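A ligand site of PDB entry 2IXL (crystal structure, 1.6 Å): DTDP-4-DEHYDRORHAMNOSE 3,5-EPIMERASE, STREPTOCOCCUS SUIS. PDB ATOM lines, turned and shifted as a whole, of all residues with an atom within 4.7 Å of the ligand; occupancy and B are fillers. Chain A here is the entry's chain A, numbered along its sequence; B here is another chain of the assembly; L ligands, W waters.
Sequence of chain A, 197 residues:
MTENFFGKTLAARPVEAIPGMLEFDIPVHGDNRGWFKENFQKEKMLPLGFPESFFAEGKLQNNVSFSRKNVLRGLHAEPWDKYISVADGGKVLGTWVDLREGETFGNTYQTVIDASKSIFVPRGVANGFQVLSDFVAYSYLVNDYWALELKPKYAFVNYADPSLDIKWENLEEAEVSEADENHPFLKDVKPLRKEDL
Water W12 bridges O10 of the ligand (2.4 Å) and NZ of Lys 151 (3.3 Å).
Water W2 bridges O10 of the ligand and NZ of Lys 151.
Water W3 bridges an oxygen (O5) of the ligand (2.7 Å) and the indole nitrogen of Trp 80 (2.8 Å).
Water W9 bridges an oxygen (O14) of the ligand and the side-chain carboxylate (OE2) of Glu 38 of chain B.
Water W6 bridges O15 of the ligand (2.8 Å) and OD1 of Asn 63 (3.0 Å).
Residues that only touch the ligand: Tyr 140 (3.4 Å), Trp 146 (3.2 Å), His 29 of chain B (3.8 Å) and Phe 36 of chain B (3.2 Å).
Hydrophobic or aromatic side chains that line the ligand: His 76, Trp 146, His 29 of chain B and Phe 36 of chain B.
The side-chain carboxylate of Glu 78 is in hydrogen-bond range of an oxygen (O4) of the ligand, 2.5 Å away.
A ring nitrogen (ND1) of His 76 lies within hydrogen-bond range of an oxygen (O4) of the ligand (2.7 Å).
A nitrogen (N2) of the ligand lies within hydrogen-bond range of the side-chain carboxylate of Glu 38 of chain B.
The side-chain amide nitrogen of Asn 127 lies within hydrogen-bond range of an oxygen (O6) of the ligand.
The side-chain amino group of Lys 82 is in hydrogen-bond range of an oxygen (O6) of the ligand (2.8 Å).
NH2 of Arg 33 of chain B is in salt-bridge range of O9 of the ligand (2.8 Å).
NH1 of Arg 73 is in salt-bridge range of O2 of the ligand (3.0 Å).
The side-chain amide oxygen (OE1) of Gln 61 sits close to an oxygen (O15) of the ligand, at 3.4 Å.
The side-chain amino group (NZ) of Lys 151 is in salt-bridge range of an oxygen (O10) of the ligand (3.99 Å).
The side-chain amino group of Lys 82 is in salt-bridge range of the side-chain carboxylate of Glu 78 (3.0 Å).
The backbone carbonyl oxygen (O) of His 76 sits at hydrogen-bond distance from the side-chain amino group (NZ) of Lys 82, at 3.2 Å.
NE2 of His 76 lies within hydrogen-bond range of OD1 of Asp 180, at 2.7 Å.
The side-chain amide oxygen of Gln 61 sits close to the side-chain carboxylate of Glu 38 of chain B.
O of Arg 73 sits at hydrogen-bond distance from N of Phe 129, 2.9 Å away.
N of His 29 of chain B is in hydrogen-bond range of O of Phe 36 of chain B.
ND2 of Asn 63 sits at hydrogen-bond distance from OE1 of Gln 61, 2.8 Å away.
N of Tyr 140 lies within hydrogen-bond range of O of Asn 63 (2.9 Å).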
ATOM      1  N   GLN A  61     -29.603 -12.716  28.319  1.00  0.00           N
ATOM      2  CA  GLN A  61     -28.740 -11.566  27.961  1.00  0.00           C
ATOM      3  C   GLN A  61     -29.538 -10.622  27.045  1.00  0.00           C
ATOM      4  O   GLN A  61     -30.292 -11.086  26.168  1.00  0.00           O
ATOM      5  CB  GLN A  61     -27.456 -12.044  27.268  1.00  0.00           C
ATOM      6  CG  GLN A  61     -26.508 -10.945  26.751  1.00  0.00           C
ATOM      7  CD  GLN A  61     -25.211 -11.465  26.180  1.00  0.00           C
ATOM      8  OE1 GLN A  61     -24.544 -10.769  25.404  1.00  0.00           O
ATOM      9  NE2 GLN A  61     -24.818 -12.662  26.566  1.00  0.00           N
ATOM     10  N   ASN A  63     -28.850  -7.468  24.460  1.00  0.00           N
ATOM     11  CA  ASN A  63     -27.875  -6.660  23.696  1.00  0.00           C
ATOM     12  C   ASN A  63     -28.556  -5.486  23.005  1.00  0.00           C
ATOM     13  O   ASN A  63     -29.742  -5.577  22.652  1.00  0.00           O
ATOM     14  CB  ASN A  63     -27.171  -7.485  22.600  1.00  0.00           C
ATOM     15  CG  ASN A  63     -26.402  -8.682  23.150  1.00  0.00           C
ATOM     16  OD1 ASN A  63     -26.372  -9.754  22.508  1.00  0.00           O
ATOM     17  ND2 ASN A  63     -25.791  -8.526  24.300  1.00  0.00           N
ATOM     18  N   ARG A  73     -25.199  -5.455   9.077  1.00  0.00           N
ATOM     19  CA  ARG A  73     -24.608  -6.426  10.017  1.00  0.00           C
ATOM     20  C   ARG A  73     -25.161  -7.825   9.694  1.00  0.00           C
ATOM     21  O   ARG A  73     -26.383  -7.986   9.564  1.00  0.00           O
ATOM     22  CB  ARG A  73     -24.938  -6.039  11.474  1.00  0.00           C
ATOM     23  CG  ARG A  73     -24.507  -4.594  11.877  1.00  0.00           C
ATOM     24  CD  ARG A  73     -24.664  -4.392  13.408  1.00  0.00           C
ATOM     25  NE  ARG A  73     -24.458  -3.000  13.856  1.00  0.00           N
ATOM     26  CZ  ARG A  73     -23.541  -2.593  14.726  1.00  0.00           C
ATOM     27  NH1 ARG A  73     -22.675  -3.435  15.276  1.00  0.00           N
ATOM     28  NH2 ARG A  73     -23.468  -1.298  15.049  1.00  0.00           N
ATOM     29  N   GLY A  74     -24.284  -8.805   9.519  1.00  0.00           N
ATOM     30  CA  GLY A  74     -24.707 -10.197   9.257  1.00  0.00           C
ATOM     31  C   GLY A  74     -23.759 -10.936   8.314  1.00  0.00           C
ATOM     32  O   GLY A  74     -22.739 -10.376   7.889  1.00  0.00           O
ATOM     33  N   HIS A  76     -25.221 -13.943  10.753  1.00  0.00           N
ATOM     34  CA  HIS A  76     -24.611 -14.612  11.914  1.00  0.00           C
ATOM     35  C   HIS A  76     -25.565 -15.626  12.551  1.00  0.00           C
ATOM     36  O   HIS A  76     -26.702 -15.273  12.887  1.00  0.00           O
ATOM     37  CB  HIS A  76     -24.229 -13.585  12.993  1.00  0.00           C
ATOM     38  CG  HIS A  76     -23.413 -12.421  12.502  1.00  0.00           C
ATOM     39  ND1 HIS A  76     -23.385 -11.211  13.160  1.00  0.00           N
ATOM     40  CD2 HIS A  76     -22.628 -12.272  11.402  1.00  0.00           C
ATOM     41  CE1 HIS A  76     -22.585 -10.373  12.513  1.00  0.00           C
ATOM     42  NE2 HIS A  76     -22.117 -10.995  11.442  1.00  0.00           N
ATOM     43  N   GLU A  78     -25.010 -17.774  15.511  1.00  0.00           N
ATOM     44  CA  GLU A  78     -24.490 -18.237  16.796  1.00  0.00           C
ATOM     45  C   GLU A  78     -25.426 -19.270  17.455  1.00  0.00           C
ATOM     46  O   GLU A  78     -26.638 -19.271  17.201  1.00  0.00           O
ATOM     47  CB  GLU A  78     -24.274 -17.054  17.734  1.00  0.00           C
ATOM     48  CG  GLU A  78     -23.184 -16.083  17.319  1.00  0.00           C
ATOM     49  CD  GLU A  78     -23.713 -14.765  16.773  1.00  0.00           C
ATOM     50  OE1 GLU A  78     -24.809 -14.755  16.176  1.00  0.00           O
ATOM     51  OE2 GLU A  78     -23.000 -13.738  16.929  1.00  0.00           O
ATOM     52  N   TRP A  80     -27.534 -19.928  19.721  1.00  0.00           N
ATOM     53  CA  TRP A  80     -28.581 -19.523  20.674  1.00  0.00           C
ATOM     54  C   TRP A  80     -29.760 -18.912  19.937  1.00  0.00           C
ATOM     55  O   TRP A  80     -29.626 -18.544  18.754  1.00  0.00           O
ATOM     56  CB  TRP A  80     -28.050 -18.565  21.768  1.00  0.00           C
ATOM     57  CG  TRP A  80     -27.266 -17.351  21.281  1.00  0.00           C
ATOM     58  CD1 TRP A  80     -27.763 -16.172  20.797  1.00  0.00           C
ATOM     59  CD2 TRP A  80     -25.839 -17.210  21.281  1.00  0.00           C
ATOM     60  NE1 TRP A  80     -26.731 -15.313  20.479  1.00  0.00           N
ATOM     61  CE2 TRP A  80     -25.537 -15.918  20.778  1.00  0.00           C
ATOM     62  CE3 TRP A  80     -24.776 -18.049  21.670  1.00  0.00           C
ATOM     63  CZ2 TRP A  80     -24.226 -15.452  20.642  1.00  0.00           C
ATOM     64  CZ3 TRP A  80     -23.478 -17.587  21.532  1.00  0.00           C
ATOM     65  CH2 TRP A  80     -23.208 -16.309  21.017  1.00  0.00           C
ATOM     66  N   LYS A  82     -32.772 -15.950  19.389  1.00  0.00           N
ATOM     67  CA  LYS A  82     -32.810 -14.472  19.433  1.00  0.00           C
ATOM     68  C   LYS A  82     -34.225 -13.931  19.291  1.00  0.00           C
ATOM     69  O   LYS A  82     -34.986 -14.387  18.442  1.00  0.00           O
ATOM     70  CB  LYS A  82     -31.927 -13.852  18.330  1.00  0.00           C
ATOM     71  CG  LYS A  82     -30.419 -14.237  18.358  1.00  0.00           C
ATOM     72  CD  LYS A  82     -29.729 -13.852  17.039  1.00  0.00           C
ATOM     73  CE  LYS A  82     -28.273 -14.283  17.022  1.00  0.00           C
ATOM     74  NZ  LYS A  82     -27.659 -14.090  15.674  1.00  0.00           N
ATOM     75  N   ASN A 127     -28.937 -14.513  11.157  1.00  0.00           N
ATOM     76  CA  ASN A 127     -29.587 -13.192  11.306  1.00  0.00           C
ATOM     77  C   ASN A 127     -28.756 -12.044  10.729  1.00  0.00           C
ATOM     78  O   ASN A 127     -27.524 -12.037  10.829  1.00  0.00           O
ATOM     79  CB  ASN A 127     -29.837 -12.940  12.805  1.00  0.00           C
ATOM     80  CG  ASN A 127     -30.580 -11.637  13.077  1.00  0.00           C
ATOM     81  OD1 ASN A 127     -31.726 -11.461  12.661  1.00  0.00           O
ATOM     82  ND2 ASN A 127     -29.937 -10.725  13.822  1.00  0.00           N
ATOM     83  N   GLY A 128     -29.437 -11.068  10.131  1.00  0.00           N
ATOM     84  CA  GLY A 128     -28.766  -9.865   9.621  1.00  0.00           C
ATOM     85  C   GLY A 128     -29.737  -8.724   9.391  1.00  0.00           C
ATOM     86  O   GLY A 128     -30.969  -8.916   9.402  1.00  0.00           O
ATOM     87  N   PHE A 129     -29.204  -7.526   9.172  1.00  0.00           N
ATOM     88  CA  PHE A 129     -30.037  -6.349   8.834  1.00  0.00           C
ATOM     89  C   PHE A 129     -29.250  -5.253   8.138  1.00  0.00           C
ATOM     90  O   PHE A 129     -28.031  -5.186   8.280  1.00  0.00           O
ATOM     91  CB  PHE A 129     -30.763  -5.775  10.072  1.00  0.00           C
ATOM     92  CG  PHE A 129     -29.829  -5.173  11.112  1.00  0.00           C
ATOM     93  CD1 PHE A 129     -29.565  -3.804  11.107  1.00  0.00           C
ATOM     94  CD2 PHE A 129     -29.254  -5.961  12.104  1.00  0.00           C
ATOM     95  CE1 PHE A 129     -28.733  -3.228  12.056  1.00  0.00           C
ATOM     96  CE2 PHE A 129     -28.415  -5.394  13.072  1.00  0.00           C
ATOM     97  CZ  PHE A 129     -28.148  -4.025  13.050  1.00  0.00           C
ATOM     98  N   TYR A 140     -32.092  -6.774  21.405  1.00  0.00           N
ATOM     99  CA  TYR A 140     -32.515  -8.171  21.344  1.00  0.00           C
ATOM    100  C   TYR A 140     -32.264  -8.952  22.630  1.00  0.00           C
ATOM    101  O   TYR A 140     -31.421  -8.563  23.444  1.00  0.00           O
ATOM    102  CB  TYR A 140     -32.021  -8.837  20.055  1.00  0.00           C
ATOM    103  CG  TYR A 140     -30.528  -8.799  19.806  1.00  0.00           C
ATOM    104  CD1 TYR A 140     -29.782  -9.973  19.850  1.00  0.00           C
ATOM    105  CD2 TYR A 140     -29.875  -7.603  19.482  1.00  0.00           C
ATOM    106  CE1 TYR A 140     -28.425  -9.949  19.627  1.00  0.00           C
ATOM    107  CE2 TYR A 140     -28.524  -7.571  19.239  1.00  0.00           C
ATOM    108  CZ  TYR A 140     -27.799  -8.747  19.315  1.00  0.00           C
ATOM    109  OH  TYR A 140     -26.436  -8.740  19.087  1.00  0.00           O
ATOM    110  N   TRP A 146     -22.188 -15.267  24.751  1.00  0.00           N
ATOM    111  CA  TRP A 146     -21.090 -15.053  23.794  1.00  0.00           C
ATOM    112  C   TRP A 146     -19.734 -14.979  24.506  1.00  0.00           C
ATOM    113  O   TRP A 146     -19.624 -14.456  25.612  1.00  0.00           O
ATOM    114  CB  TRP A 146     -21.371 -13.721  23.074  1.00  0.00           C
ATOM    115  CG  TRP A 146     -20.384 -13.284  22.014  1.00  0.00           C
ATOM    116  CD1 TRP A 146     -20.477 -13.522  20.663  1.00  0.00           C
ATOM    117  CD2 TRP A 146     -19.232 -12.443  22.192  1.00  0.00           C
ATOM    118  NE1 TRP A 146     -19.432 -12.919  20.000  1.00  0.00           N
ATOM    119  CE2 TRP A 146     -18.643 -12.261  20.916  1.00  0.00           C
ATOM    120  CE3 TRP A 146     -18.624 -11.857  23.308  1.00  0.00           C
ATOM    121  CZ2 TRP A 146     -17.484 -11.499  20.726  1.00  0.00           C
ATOM    122  CZ3 TRP A 146     -17.464 -11.103  23.124  1.00  0.00           C
ATOM    123  CH2 TRP A 146     -16.912 -10.920  21.841  1.00  0.00           C
ATOM    124  N   LYS A 151     -15.678 -17.634  19.078  1.00  0.00           N
ATOM    125  CA  LYS A 151     -16.123 -17.171  17.760  1.00  0.00           C
ATOM    126  C   LYS A 151     -15.781 -18.118  16.588  1.00  0.00           C
ATOM    127  O   LYS A 151     -16.609 -18.319  15.697  1.00  0.00           O
ATOM    128  CB  LYS A 151     -15.674 -15.721  17.484  1.00  0.00           C
ATOM    129  CG  LYS A 151     -16.668 -14.910  16.667  1.00  0.00           C
ATOM    130  CD  LYS A 151     -16.241 -13.458  16.540  1.00  0.00           C
ATOM    131  CE  LYS A 151     -16.774 -12.832  15.248  1.00  0.00           C
ATOM    132  NZ  LYS A 151     -18.229 -12.640  15.229  1.00  0.00           N
ATOM    133  N   ASP A 180     -17.340  -9.110   8.872  1.00  0.00           N
ATOM    134  CA  ASP A 180     -18.421  -9.414   7.938  1.00  0.00           C
ATOM    135  C   ASP A 180     -17.982  -9.455   6.484  1.00  0.00           C
ATOM    136  O   ASP A 180     -18.610 -10.101   5.647  1.00  0.00           O
ATOM    137  CB  ASP A 180     -19.612  -8.467   8.151  1.00  0.00           C
ATOM    138  CG  ASP A 180     -20.450  -8.846   9.363  1.00  0.00           C
ATOM    139  OD1 ASP A 180     -20.247  -9.967   9.863  1.00  0.00           O
ATOM    140  OD2 ASP A 180     -21.317  -8.048   9.791  1.00  0.00           O
ATOM    141  N   HIS B  29     -18.882  -0.440  23.252  1.00  0.00           N
ATOM    142  CA  HIS B  29     -17.795  -0.629  22.284  1.00  0.00           C
ATOM    143  C   HIS B  29     -18.148   0.081  20.979  1.00  0.00           C
ATOM    144  O   HIS B  29     -19.131  -0.280  20.337  1.00  0.00           O
ATOM    145  CB  HIS B  29     -17.611  -2.134  22.035  1.00  0.00           C
ATOM    146  CG  HIS B  29     -17.323  -2.908  23.275  1.00  0.00           C
ATOM    147  ND1 HIS B  29     -18.237  -3.783  23.834  1.00  0.00           N
ATOM    148  CD2 HIS B  29     -16.248  -2.919  24.097  1.00  0.00           C
ATOM    149  CE1 HIS B  29     -17.719  -4.315  24.927  1.00  0.00           C
ATOM    150  NE2 HIS B  29     -16.512  -3.811  25.111  1.00  0.00           N
ATOM    151  N   ARG B  33     -19.379   1.689  12.495  1.00  0.00           N
ATOM    152  CA  ARG B  33     -20.806   1.467  12.237  1.00  0.00           C
ATOM    153  C   ARG B  33     -21.705   2.201  13.244  1.00  0.00           C
ATOM    154  O   ARG B  33     -22.873   2.488  12.951  1.00  0.00           O
ATOM    155  CB  ARG B  33     -21.126  -0.042  12.258  1.00  0.00           C
ATOM    156  CG  ARG B  33     -20.514  -0.853  11.102  1.00  0.00           C
ATOM    157  CD  ARG B  33     -20.633  -2.354  11.363  1.00  0.00           C
ATOM    158  NE  ARG B  33     -20.057  -2.757  12.647  1.00  0.00           N
ATOM    159  CZ  ARG B  33     -20.158  -3.965  13.182  1.00  0.00           C
ATOM    160  NH1 ARG B  33     -20.794  -4.947  12.557  1.00  0.00           N
ATOM    161  NH2 ARG B  33     -19.602  -4.202  14.371  1.00  0.00           N
ATOM    162  N   PHE B  36     -22.033  -1.004  20.218  1.00  0.00           N
ATOM    163  CA  PHE B  36     -22.636  -2.252  20.724  1.00  0.00           C
ATOM    164  C   PHE B  36     -22.431  -2.325  22.245  1.00  0.00           C
ATOM    165  O   PHE B  36     -21.351  -2.003  22.726  1.00  0.00           O
ATOM    166  CB  PHE B  36     -21.974  -3.470  20.064  1.00  0.00           C
ATOM    167  CG  PHE B  36     -22.607  -4.780  20.436  1.00  0.00           C
ATOM    168  CD1 PHE B  36     -23.482  -5.406  19.561  1.00  0.00           C
ATOM    169  CD2 PHE B  36     -22.341  -5.389  21.674  1.00  0.00           C
ATOM    170  CE1 PHE B  36     -24.091  -6.626  19.895  1.00  0.00           C
ATOM    171  CE2 PHE B  36     -22.962  -6.607  22.029  1.00  0.00           C
ATOM    172  CZ  PHE B  36     -23.842  -7.210  21.135  1.00  0.00           C
ATOM    173  N   GLU B  38     -23.568  -5.105  25.786  1.00  0.00           N
ATOM    174  CA  GLU B  38     -24.359  -6.084  26.544  1.00  0.00           C
ATOM    175  C   GLU B  38     -25.088  -5.304  27.653  1.00  0.00           C
ATOM    176  O   GLU B  38     -24.514  -4.999  28.704  1.00  0.00           O
ATOM    177  CB  GLU B  38     -23.482  -7.191  27.167  1.00  0.00           C
ATOM    178  CG  GLU B  38     -22.519  -7.882  26.184  1.00  0.00           C
ATOM    179  CD  GLU B  38     -21.722  -9.043  26.804  1.00  0.00           C
ATOM    180  OE1 GLU B  38     -21.548  -9.089  28.047  1.00  0.00           O
ATOM    181  OE2 GLU B  38     -21.260  -9.924  26.038  1.00  0.00           O
HETATM  182  O1  LIG L   1     -21.550  -7.378  14.018  1.00  0.00           O
HETATM  183  P1  LIG L   1     -22.269  -7.295  15.450  1.00  0.00           P
HETATM  184  O2  LIG L   1     -23.459  -6.272  15.803  1.00  0.00           O
HETATM  185  O3  LIG L   1     -22.732  -8.782  15.860  1.00  0.00           O
HETATM  186  C1  LIG L   1     -24.106  -9.146  15.958  1.00  0.00           C
HETATM  187  C2  LIG L   1     -24.172 -10.516  16.621  1.00  0.00           C
HETATM  188  O4  LIG L   1     -23.356 -11.440  15.891  1.00  0.00           O
HETATM  189  C3  LIG L   1     -25.627 -10.970  16.657  1.00  0.00           C
HETATM  190  O5  LIG L   1     -25.714 -12.276  17.245  1.00  0.00           O
HETATM  191  C4  LIG L   1     -26.239 -10.939  15.244  1.00  0.00           C
HETATM  192  O6  LIG L   1     -27.625 -11.286  15.333  1.00  0.00           O
HETATM  193  C5  LIG L   1     -26.069  -9.557  14.607  1.00  0.00           C
HETATM  194  O7  LIG L   1     -24.691  -9.189  14.640  1.00  0.00           O
HETATM  195  C6  LIG L   1     -26.574  -9.491  13.168  1.00  0.00           C
HETATM  196  O8  LIG L   1     -21.137  -7.051  16.573  1.00  0.00           O
HETATM  197  P2  LIG L   1     -19.606  -7.519  16.542  1.00  0.00           P
HETATM  198  O9  LIG L   1     -18.769  -6.686  15.438  1.00  0.00           O
HETATM  199  O10 LIG L   1     -19.480  -9.114  16.624  1.00  0.00           O
HETATM  200  O11 LIG L   1     -19.168  -6.991  18.003  1.00  0.00           O
HETATM  201  C7  LIG L   1     -19.123  -5.589  18.335  1.00  0.00           C
HETATM  202  C8  LIG L   1     -18.448  -5.400  19.686  1.00  0.00           C
HETATM  203  O12 LIG L   1     -19.269  -5.910  20.751  1.00  0.00           O
HETATM  204  C9  LIG L   1     -17.118  -6.132  19.803  1.00  0.00           C
HETATM  205  O13 LIG L   1     -16.166  -5.294  20.476  1.00  0.00           O
HETATM  206  C10 LIG L   1     -17.394  -7.373  20.633  1.00  0.00           C
HETATM  207  C11 LIG L   1     -18.586  -6.947  21.481  1.00  0.00           C
HETATM  208  N1  LIG L   1     -19.607  -7.996  21.787  1.00  0.00           N
HETATM  209  C12 LIG L   1     -19.870  -8.309  23.078  1.00  0.00           C
HETATM  210  O14 LIG L   1     -19.217  -7.752  24.087  1.00  0.00           O
HETATM  211  N2  LIG L   1     -20.811  -9.216  23.398  1.00  0.00           N
HETATM  212  C13 LIG L   1     -21.516  -9.820  22.421  1.00  0.00           C
HETATM  213  O15 LIG L   1     -22.430 -10.705  22.763  1.00  0.00           O
HETATM  214  C14 LIG L   1     -21.276  -9.530  21.091  1.00  0.00           C
HETATM  215  C15 LIG L   1     -22.060 -10.200  19.970  1.00  0.00           C
HETATM  216  C16 LIG L   1     -20.298  -8.581  20.784  1.00  0.00           C
HETATM  217  O   HOH W   1     -14.659  -6.158  23.017  1.00  0.00           O
HETATM  218  O   HOH W   2     -20.527 -11.126  15.303  1.00  0.00           O
HETATM  219  O   HOH W   3     -26.353 -12.579  19.844  1.00  0.00           O
HETATM  220  O   HOH W   4     -19.036  -6.125  26.810  1.00  0.00           O
HETATM  221  O   HOH W   5     -16.039  -2.904  18.661  1.00  0.00           O
HETATM  222  O   HOH W   6     -24.677 -12.152  21.984  1.00  0.00           O
HETATM  223  O   HOH W   7     -19.074  -8.244  12.730  1.00  0.00           O
HETATM  224  O   HOH W   8     -26.272  -5.908  16.310  1.00  0.00           O
HETATM  225  O   HOH W   9     -18.265  -8.665  26.534  1.00  0.00           O
HETATM  226  O   HOH W  10     -16.416  -7.700  24.788  1.00  0.00           O
HETATM  227  O   HOH W  11     -18.916  -2.222  18.312  1.00  0.00           O
HETATM  228  O   HOH W  12     -17.428 -10.251  17.312  1.00  0.00           O
HETATM  229  O   HOH W  13     -16.086  -6.260  15.189  1.00  0.00           O
